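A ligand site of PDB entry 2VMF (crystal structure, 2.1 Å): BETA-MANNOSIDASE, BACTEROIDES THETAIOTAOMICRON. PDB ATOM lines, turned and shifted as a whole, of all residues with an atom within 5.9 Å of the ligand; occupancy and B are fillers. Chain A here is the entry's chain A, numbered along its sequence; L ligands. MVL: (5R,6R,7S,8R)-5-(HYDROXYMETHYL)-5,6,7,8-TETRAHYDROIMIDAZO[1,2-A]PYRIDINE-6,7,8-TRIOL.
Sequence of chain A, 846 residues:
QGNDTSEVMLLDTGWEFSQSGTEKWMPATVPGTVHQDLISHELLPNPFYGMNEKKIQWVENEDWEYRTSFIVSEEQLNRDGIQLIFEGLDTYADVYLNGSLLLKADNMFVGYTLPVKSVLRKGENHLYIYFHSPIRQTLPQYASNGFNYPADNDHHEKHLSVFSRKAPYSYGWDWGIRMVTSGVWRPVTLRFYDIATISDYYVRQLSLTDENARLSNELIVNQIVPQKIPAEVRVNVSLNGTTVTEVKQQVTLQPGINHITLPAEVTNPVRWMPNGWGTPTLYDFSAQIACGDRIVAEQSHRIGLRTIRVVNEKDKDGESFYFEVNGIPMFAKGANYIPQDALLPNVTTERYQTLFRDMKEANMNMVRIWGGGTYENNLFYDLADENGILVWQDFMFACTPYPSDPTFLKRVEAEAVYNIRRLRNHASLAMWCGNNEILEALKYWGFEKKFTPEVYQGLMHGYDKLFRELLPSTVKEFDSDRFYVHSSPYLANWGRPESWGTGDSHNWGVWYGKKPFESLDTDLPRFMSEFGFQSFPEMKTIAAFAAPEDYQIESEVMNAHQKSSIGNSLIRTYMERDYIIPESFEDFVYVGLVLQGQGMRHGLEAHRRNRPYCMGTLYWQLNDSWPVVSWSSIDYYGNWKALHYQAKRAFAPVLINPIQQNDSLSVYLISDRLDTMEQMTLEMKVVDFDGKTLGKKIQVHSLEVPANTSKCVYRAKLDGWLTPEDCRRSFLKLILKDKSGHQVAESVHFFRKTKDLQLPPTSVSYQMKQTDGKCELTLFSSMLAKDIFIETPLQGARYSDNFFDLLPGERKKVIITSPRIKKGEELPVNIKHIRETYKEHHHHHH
OD2 of Asp 174 is in hydrogen-bond range of O6 of the ligand (2.6 Å). ND2 of Asn 436 lies within hydrogen-bond range of O2 of the ligand (3.0 Å). O3 of the ligand sits at hydrogen-bond distance from NE1 of Trp 173 (3.2 Å). A nitrogen (N1) of the ligand is in hydrogen-bond range of the side-chain carboxylate (OE2) of Glu 437 (2.7 Å). NE1 of Trp 175 is in hydrogen-bond range of O4 of the ligand (2.9 Å). OE2 of Glu 530 lies within hydrogen-bond range of O2 of the ligand (2.6 Å). An oxygen (O2) of the ligand sits at hydrogen-bond distance from the indole nitrogen (NE1) of Trp 370, at 3.2 Å. OH of Tyr 512 is in hydrogen-bond range of O6 of the ligand (2.7 Å). The indole nitrogen of Trp 508 sits close to a nitrogen (N1) of the ligand (3.3 Å).
A ring nitrogen (ND1) of His 506 lies within hydrogen-bond range of the side-chain carboxylate of Glu 530 (3.1 Å). The side-chain carboxylate of Glu 437 sits at hydrogen-bond distance from the side-chain sulfur of Cys 399 (3.7 Å). The guanidinium group (NH2) of Arg 368 is in hydrogen-bond range of the side-chain amide oxygen (OD1) of Asn 436, at 2.8 Å. N of Cys 399 lies within hydrogen-bond range of O of Asn 436 (2.7 Å). The side-chain carboxylate (OE2) of Glu 530 lies within salt-bridge range of the guanidinium group (NH1) of Arg 368 (2.9 Å). The backbone NH of Asp 174 sits at hydrogen-bond distance from the side-chain amide oxygen of Asn 153, at 3.2 Å. The side-chain carboxylate (OE2) of Glu 437 is in hydrogen-bond range of a ring nitrogen (ND1) of His 506 (2.7 Å). NE1 of Trp 508 lies within hydrogen-bond range of OE1 of Glu 530 (2.8 Å).
Cys 399 touches the ligand (SG to O3, 3.8 Å). Trp 620 touches the ligand (CZ2 to O4, 3.3 Å). Trp 631 touches the ligand (CZ2 to C6, 3.5 Å). The nearest printed residue that does not touch the ligand is His 506 (4.6 Å).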
ATOM      1  N   ASN A 153      -0.453  -4.921  30.424  1.00  0.00           N
ATOM      2  CA  ASN A 153      -0.247  -4.215  29.135  1.00  0.00           C
ATOM      3  C   ASN A 153       1.122  -4.469  28.565  1.00  0.00           C
ATOM      4  O   ASN A 153       1.394  -4.071  27.446  1.00  0.00           O
ATOM      5  CB  ASN A 153      -0.534  -2.742  29.274  1.00  0.00           C
ATOM      6  CG  ASN A 153      -1.994  -2.452  29.370  1.00  0.00           C
ATOM      7  OD1 ASN A 153      -2.705  -2.510  28.379  1.00  0.00           O
ATOM      8  ND2 ASN A 153      -2.453  -2.146  30.570  1.00  0.00           N
ATOM      9  N   TRP A 173       0.618  -1.745  24.788  1.00  0.00           N
ATOM     10  CA  TRP A 173      -0.531  -1.248  25.546  1.00  0.00           C
ATOM     11  C   TRP A 173      -1.825  -1.700  24.843  1.00  0.00           C
ATOM     12  O   TRP A 173      -1.745  -2.351  23.789  1.00  0.00           O
ATOM     13  CB  TRP A 173      -0.512   0.285  25.764  1.00  0.00           C
ATOM     14  CG  TRP A 173      -1.072   0.630  27.193  1.00  0.00           C
ATOM     15  CD1 TRP A 173      -2.344   1.021  27.497  1.00  0.00           C
ATOM     16  CD2 TRP A 173      -0.360   0.584  28.450  1.00  0.00           C
ATOM     17  NE1 TRP A 173      -2.482   1.219  28.868  1.00  0.00           N
ATOM     18  CE2 TRP A 173      -1.286   0.941  29.476  1.00  0.00           C
ATOM     19  CE3 TRP A 173       0.962   0.259  28.813  1.00  0.00           C
ATOM     20  CZ2 TRP A 173      -0.925   0.979  30.831  1.00  0.00           C
ATOM     21  CZ3 TRP A 173       1.314   0.286  30.162  1.00  0.00           C
ATOM     22  CH2 TRP A 173       0.357   0.648  31.168  1.00  0.00           C
ATOM     23  N   ASP A 174      -3.004  -1.349  25.405  1.00  0.00           N
ATOM     24  CA  ASP A 174      -4.278  -1.850  24.848  1.00  0.00           C
ATOM     25  C   ASP A 174      -4.746  -0.970  23.655  1.00  0.00           C
ATOM     26  O   ASP A 174      -5.821  -1.195  23.102  1.00  0.00           O
ATOM     27  CB  ASP A 174      -5.346  -2.083  25.945  1.00  0.00           C
ATOM     28  CG  ASP A 174      -5.702  -0.766  26.718  1.00  0.00           C
ATOM     29  OD1 ASP A 174      -5.271   0.318  26.305  1.00  0.00           O
ATOM     30  OD2 ASP A 174      -6.372  -0.821  27.739  1.00  0.00           O
ATOM     31  N   TRP A 175      -3.887  -0.048  23.219  1.00  0.00           N
ATOM     32  CA  TRP A 175      -4.058   0.700  21.980  1.00  0.00           C
ATOM     33  C   TRP A 175      -2.739   0.769  21.244  1.00  0.00           C
ATOM     34  O   TRP A 175      -2.603   1.495  20.262  1.00  0.00           O
ATOM     35  CB  TRP A 175      -4.599   2.155  22.273  1.00  0.00           C
ATOM     36  CG  TRP A 175      -3.931   2.767  23.524  1.00  0.00           C
ATOM     37  CD1 TRP A 175      -4.502   2.924  24.740  1.00  0.00           C
ATOM     38  CD2 TRP A 175      -2.555   3.224  23.673  1.00  0.00           C
ATOM     39  NE1 TRP A 175      -3.622   3.505  25.623  1.00  0.00           N
ATOM     40  CE2 TRP A 175      -2.408   3.671  25.004  1.00  0.00           C
ATOM     41  CE3 TRP A 175      -1.447   3.321  22.784  1.00  0.00           C
ATOM     42  CZ2 TRP A 175      -1.180   4.186  25.510  1.00  0.00           C
ATOM     43  CZ3 TRP A 175      -0.188   3.844  23.288  1.00  0.00           C
ATOM     44  CH2 TRP A 175      -0.104   4.281  24.630  1.00  0.00           C
ATOM     45  N   ARG A 368      -4.131  15.873  30.336  1.00  0.00           N
ATOM     46  CA  ARG A 368      -3.416  15.002  31.235  1.00  0.00           C
ATOM     47  C   ARG A 368      -2.351  14.202  30.456  1.00  0.00           C
ATOM     48  O   ARG A 368      -2.673  13.551  29.440  1.00  0.00           O
ATOM     49  CB  ARG A 368      -4.420  14.058  31.962  1.00  0.00           C
ATOM     50  CG  ARG A 368      -3.685  12.985  32.733  1.00  0.00           C
ATOM     51  CD  ARG A 368      -4.621  12.232  33.714  1.00  0.00           C
ATOM     52  NE  ARG A 368      -3.952  11.069  34.320  1.00  0.00           N
ATOM     53  CZ  ARG A 368      -4.410   9.825  34.305  1.00  0.00           C
ATOM     54  NH1 ARG A 368      -5.559   9.533  33.643  1.00  0.00           N
ATOM     55  NH2 ARG A 368      -3.690   8.865  34.911  1.00  0.00           N
ATOM     56  N   TRP A 370      -0.612  11.223  30.615  1.00  0.00           N
ATOM     57  CA  TRP A 370      -0.872   9.998  31.364  1.00  0.00           C
ATOM     58  C   TRP A 370       0.381   9.172  31.647  1.00  0.00           C
ATOM     59  O   TRP A 370       1.322   9.142  30.838  1.00  0.00           O
ATOM     60  CB  TRP A 370      -1.915   9.232  30.539  1.00  0.00           C
ATOM     61  CG  TRP A 370      -2.061   7.757  30.755  1.00  0.00           C
ATOM     62  CD1 TRP A 370      -2.924   7.162  31.599  1.00  0.00           C
ATOM     63  CD2 TRP A 370      -1.420   6.703  30.016  1.00  0.00           C
ATOM     64  NE1 TRP A 370      -2.844   5.792  31.476  1.00  0.00           N
ATOM     65  CE2 TRP A 370      -1.936   5.488  30.498  1.00  0.00           C
ATOM     66  CE3 TRP A 370      -0.465   6.686  28.980  1.00  0.00           C
ATOM     67  CZ2 TRP A 370      -1.506   4.243  30.012  1.00  0.00           C
ATOM     68  CZ3 TRP A 370      -0.038   5.453  28.511  1.00  0.00           C
ATOM     69  CH2 TRP A 370      -0.573   4.245  29.022  1.00  0.00           C
ATOM     70  N   ALA A 398       2.198   3.163  35.634  1.00  0.00           N
ATOM     71  CA  ALA A 398       0.779   2.914  35.241  1.00  0.00           C
ATOM     72  C   ALA A 398       0.310   1.492  35.467  1.00  0.00           C
ATOM     73  O   ALA A 398       0.972   0.536  35.005  1.00  0.00           O
ATOM     74  CB  ALA A 398       0.535   3.297  33.757  1.00  0.00           C
ATOM     75  N   CYS A 399      -0.805   1.358  36.163  1.00  0.00           N
ATOM     76  CA  CYS A 399      -1.639   0.117  36.163  1.00  0.00           C
ATOM     77  C   CYS A 399      -1.091  -1.096  36.826  1.00  0.00           C
ATOM     78  O   CYS A 399      -1.773  -2.149  36.860  1.00  0.00           O
ATOM     79  CB  CYS A 399      -1.986  -0.293  34.736  1.00  0.00           C
ATOM     80  SG  CYS A 399      -2.978   0.912  33.857  1.00  0.00           S
ATOM     81  N   ASN A 436      -0.924   6.194  37.351  1.00  0.00           N
ATOM     82  CA  ASN A 436      -2.212   5.827  36.847  1.00  0.00           C
ATOM     83  C   ASN A 436      -2.762   4.543  37.408  1.00  0.00           C
ATOM     84  O   ASN A 436      -2.196   3.458  37.145  1.00  0.00           O
ATOM     85  CB  ASN A 436      -2.145   5.734  35.299  1.00  0.00           C
ATOM     86  CG  ASN A 436      -3.440   5.336  34.704  1.00  0.00           C
ATOM     87  OD1 ASN A 436      -4.393   6.108  34.760  1.00  0.00           O
ATOM     88  ND2 ASN A 436      -3.516   4.110  34.136  1.00  0.00           N
ATOM     89  N   GLU A 437      -3.859   4.642  38.177  1.00  0.00           N
ATOM     90  CA  GLU A 437      -4.671   3.458  38.591  1.00  0.00           C
ATOM     91  C   GLU A 437      -3.960   2.357  39.391  1.00  0.00           C
ATOM     92  O   GLU A 437      -4.487   1.241  39.474  1.00  0.00           O
ATOM     93  CB  GLU A 437      -5.380   2.767  37.376  1.00  0.00           C
ATOM     94  CG  GLU A 437      -6.406   3.631  36.703  1.00  0.00           C
ATOM     95  CD  GLU A 437      -6.849   3.114  35.350  1.00  0.00           C
ATOM     96  OE1 GLU A 437      -6.311   2.090  34.811  1.00  0.00           O
ATOM     97  OE2 GLU A 437      -7.753   3.769  34.822  1.00  0.00           O
ATOM     98  N   HIS A 506     -12.221   7.659  37.234  1.00  0.00           N
ATOM     99  CA  HIS A 506     -12.115   7.039  35.905  1.00  0.00           C
ATOM    100  C   HIS A 506     -13.383   6.230  35.730  1.00  0.00           C
ATOM    101  O   HIS A 506     -13.471   5.092  36.208  1.00  0.00           O
ATOM    102  CB  HIS A 506     -10.879   6.101  35.812  1.00  0.00           C
ATOM    103  CG  HIS A 506      -9.564   6.829  35.951  1.00  0.00           C
ATOM    104  ND1 HIS A 506      -8.345   6.253  35.633  1.00  0.00           N
ATOM    105  CD2 HIS A 506      -9.295   8.095  36.356  1.00  0.00           C
ATOM    106  CE1 HIS A 506      -7.380   7.116  35.895  1.00  0.00           C
ATOM    107  NE2 HIS A 506      -7.924   8.245  36.325  1.00  0.00           N
ATOM    108  N   TRP A 508     -15.115   3.815  33.984  1.00  0.00           N
ATOM    109  CA  TRP A 508     -15.064   2.823  32.941  1.00  0.00           C
ATOM    110  C   TRP A 508     -16.266   1.874  33.016  1.00  0.00           C
ATOM    111  O   TRP A 508     -16.262   0.800  32.449  1.00  0.00           O
ATOM    112  CB  TRP A 508     -13.702   2.117  32.923  1.00  0.00           C
ATOM    113  CG  TRP A 508     -12.696   3.075  32.406  1.00  0.00           C
ATOM    114  CD1 TRP A 508     -11.857   3.867  33.141  1.00  0.00           C
ATOM    115  CD2 TRP A 508     -12.505   3.419  31.047  1.00  0.00           C
ATOM    116  NE1 TRP A 508     -11.107   4.675  32.283  1.00  0.00           N
ATOM    117  CE2 TRP A 508     -11.499   4.411  30.994  1.00  0.00           C
ATOM    118  CE3 TRP A 508     -13.082   2.961  29.846  1.00  0.00           C
ATOM    119  CZ2 TRP A 508     -11.016   4.908  29.771  1.00  0.00           C
ATOM    120  CZ3 TRP A 508     -12.610   3.476  28.621  1.00  0.00           C
ATOM    121  CH2 TRP A 508     -11.607   4.450  28.604  1.00  0.00           C
ATOM    122  N   TRP A 511     -18.236   1.521  28.575  1.00  0.00           N
ATOM    123  CA  TRP A 511     -17.222   0.683  27.914  1.00  0.00           C
ATOM    124  C   TRP A 511     -17.026  -0.656  28.671  1.00  0.00           C
ATOM    125  O   TRP A 511     -17.743  -1.580  28.370  1.00  0.00           O
ATOM    126  CB  TRP A 511     -15.902   1.435  27.561  1.00  0.00           C
ATOM    127  CG  TRP A 511     -14.939   0.569  26.743  1.00  0.00           C
ATOM    128  CD1 TRP A 511     -13.827  -0.042  27.216  1.00  0.00           C
ATOM    129  CD2 TRP A 511     -15.022   0.240  25.327  1.00  0.00           C
ATOM    130  NE1 TRP A 511     -13.195  -0.715  26.191  1.00  0.00           N
ATOM    131  CE2 TRP A 511     -13.924  -0.589  25.035  1.00  0.00           C
ATOM    132  CE3 TRP A 511     -15.933   0.525  24.309  1.00  0.00           C
ATOM    133  CZ2 TRP A 511     -13.697  -1.111  23.750  1.00  0.00           C
ATOM    134  CZ3 TRP A 511     -15.724   0.005  23.045  1.00  0.00           C
ATOM    135  CH2 TRP A 511     -14.609  -0.827  22.769  1.00  0.00           C
ATOM    136  N   TYR A 512     -16.124  -0.723  29.673  1.00  0.00           N
ATOM    137  CA  TYR A 512     -15.908  -1.972  30.432  1.00  0.00           C
ATOM    138  C   TYR A 512     -17.108  -2.448  31.193  1.00  0.00           C
ATOM    139  O   TYR A 512     -17.314  -3.628  31.236  1.00  0.00           O
ATOM    140  CB  TYR A 512     -14.647  -2.008  31.344  1.00  0.00           C
ATOM    141  CG  TYR A 512     -13.373  -1.897  30.573  1.00  0.00           C
ATOM    142  CD1 TYR A 512     -13.027  -2.857  29.639  1.00  0.00           C
ATOM    143  CD2 TYR A 512     -12.534  -0.803  30.723  1.00  0.00           C
ATOM    144  CE1 TYR A 512     -11.911  -2.749  28.889  1.00  0.00           C
ATOM    145  CE2 TYR A 512     -11.380  -0.677  29.977  1.00  0.00           C
ATOM    146  CZ  TYR A 512     -11.075  -1.638  29.063  1.00  0.00           C
ATOM    147  OH  TYR A 512      -9.960  -1.553  28.305  1.00  0.00           O
ATOM    148  N   GLU A 530     -10.963  10.393  33.579  1.00  0.00           N
ATOM    149  CA  GLU A 530     -11.002   9.500  32.409  1.00  0.00           C
ATOM    150  C   GLU A 530     -12.410   9.027  32.194  1.00  0.00           C
ATOM    151  O   GLU A 530     -13.071   8.634  33.155  1.00  0.00           O
ATOM    152  CB  GLU A 530     -10.158   8.191  32.575  1.00  0.00           C
ATOM    153  CG  GLU A 530      -8.644   8.345  32.557  1.00  0.00           C
ATOM    154  CD  GLU A 530      -7.915   7.017  32.565  1.00  0.00           C
ATOM    155  OE1 GLU A 530      -8.576   5.958  32.533  1.00  0.00           O
ATOM    156  OE2 GLU A 530      -6.656   7.045  32.604  1.00  0.00           O
ATOM    157  N   TRP A 620     -10.805   9.935  27.675  1.00  0.00           N
ATOM    158  CA  TRP A 620      -9.832   8.983  27.234  1.00  0.00           C
ATOM    159  C   TRP A 620     -10.240   8.565  25.781  1.00  0.00           C
ATOM    160  O   TRP A 620     -11.236   7.889  25.619  1.00  0.00           O
ATOM    161  CB  TRP A 620      -9.809   7.759  28.198  1.00  0.00           C
ATOM    162  CG  TRP A 620      -8.710   6.919  27.718  1.00  0.00           C
ATOM    163  CD1 TRP A 620      -8.759   5.992  26.704  1.00  0.00           C
ATOM    164  CD2 TRP A 620      -7.352   7.000  28.147  1.00  0.00           C
ATOM    165  NE1 TRP A 620      -7.495   5.470  26.488  1.00  0.00           N
ATOM    166  CE2 TRP A 620      -6.613   6.082  27.351  1.00  0.00           C
ATOM    167  CE3 TRP A 620      -6.686   7.758  29.128  1.00  0.00           C
ATOM    168  CZ2 TRP A 620      -5.230   5.920  27.498  1.00  0.00           C
ATOM    169  CZ3 TRP A 620      -5.296   7.571  29.294  1.00  0.00           C
ATOM    170  CH2 TRP A 620      -4.581   6.668  28.485  1.00  0.00           C
ATOM    171  N   GLN A 621      -9.482   8.918  24.749  1.00  0.00           N
ATOM    172  CA  GLN A 621      -8.149   9.511  24.848  1.00  0.00           C
ATOM    173  C   GLN A 621      -8.030  10.543  23.704  1.00  0.00           C
ATOM    174  O   GLN A 621      -8.835  10.480  22.742  1.00  0.00           O
ATOM    175  CB  GLN A 621      -7.086   8.390  24.691  1.00  0.00           C
ATOM    176  CG  GLN A 621      -7.018   7.739  23.246  1.00  0.00           C
ATOM    177  CD  GLN A 621      -6.289   6.382  23.236  1.00  0.00           C
ATOM    178  OE1 GLN A 621      -6.804   5.400  23.729  1.00  0.00           O
ATOM    179  NE2 GLN A 621      -5.110   6.340  22.669  1.00  0.00           N
ATOM    180  N   TRP A 631      -9.599   4.508  21.548  1.00  0.00           N
ATOM    181  CA  TRP A 631     -10.482   5.458  22.184  1.00  0.00           C
ATOM    182  C   TRP A 631     -10.216   6.898  21.726  1.00  0.00           C
ATOM    183  O   TRP A 631     -10.883   7.779  22.191  1.00  0.00           O
ATOM    184  CB  TRP A 631     -10.345   5.373  23.719  1.00  0.00           C
ATOM    185  CG  TRP A 631     -10.647   3.993  24.253  1.00  0.00           C
ATOM    186  CD1 TRP A 631     -11.797   3.581  24.855  1.00  0.00           C
ATOM    187  CD2 TRP A 631      -9.761   2.848  24.263  1.00  0.00           C
ATOM    188  NE1 TRP A 631     -11.716   2.245  25.195  1.00  0.00           N
ATOM    189  CE2 TRP A 631     -10.465   1.777  24.831  1.00  0.00           C
ATOM    190  CE3 TRP A 631      -8.432   2.636  23.806  1.00  0.00           C
ATOM    191  CZ2 TRP A 631      -9.886   0.498  24.995  1.00  0.00           C
ATOM    192  CZ3 TRP A 631      -7.872   1.332  23.936  1.00  0.00           C
ATOM    193  CH2 TRP A 631      -8.595   0.303  24.521  1.00  0.00           C
HETATM  194  C1  MVL L   1      -7.539   3.398  31.119  1.00  0.00           C
HETATM  195  N10 MVL L   1      -8.157   2.797  30.120  1.00  0.00           N
HETATM  196  C3  MVL L   1      -5.360   3.489  29.990  1.00  0.00           C
HETATM  197  C4  MVL L   1      -6.070   2.558  28.964  1.00  0.00           C
HETATM  198  C5  MVL L   1      -7.556   2.858  28.771  1.00  0.00           C
HETATM  199  C6  MVL L   1      -8.265   1.985  27.742  1.00  0.00           C
HETATM  200  C7  MVL L   1      -9.226   2.252  31.906  1.00  0.00           C
HETATM  201  C8  MVL L   1      -9.133   1.971  30.587  1.00  0.00           C
HETATM  202  N1  MVL L   1      -8.214   3.083  32.232  1.00  0.00           N
HETATM  203  O3  MVL L   1      -4.493   2.711  30.818  1.00  0.00           O
HETATM  204  O2  MVL L   1      -5.751   4.609  32.174  1.00  0.00           O
HETATM  205  O4  MVL L   1      -5.450   2.631  27.670  1.00  0.00           O
HETATM  206  C2  MVL L   1      -6.330   4.253  30.915  1.00  0.00           C
HETATM  207  O6  MVL L   1      -8.409   0.651  28.214  1.00  0.00           O
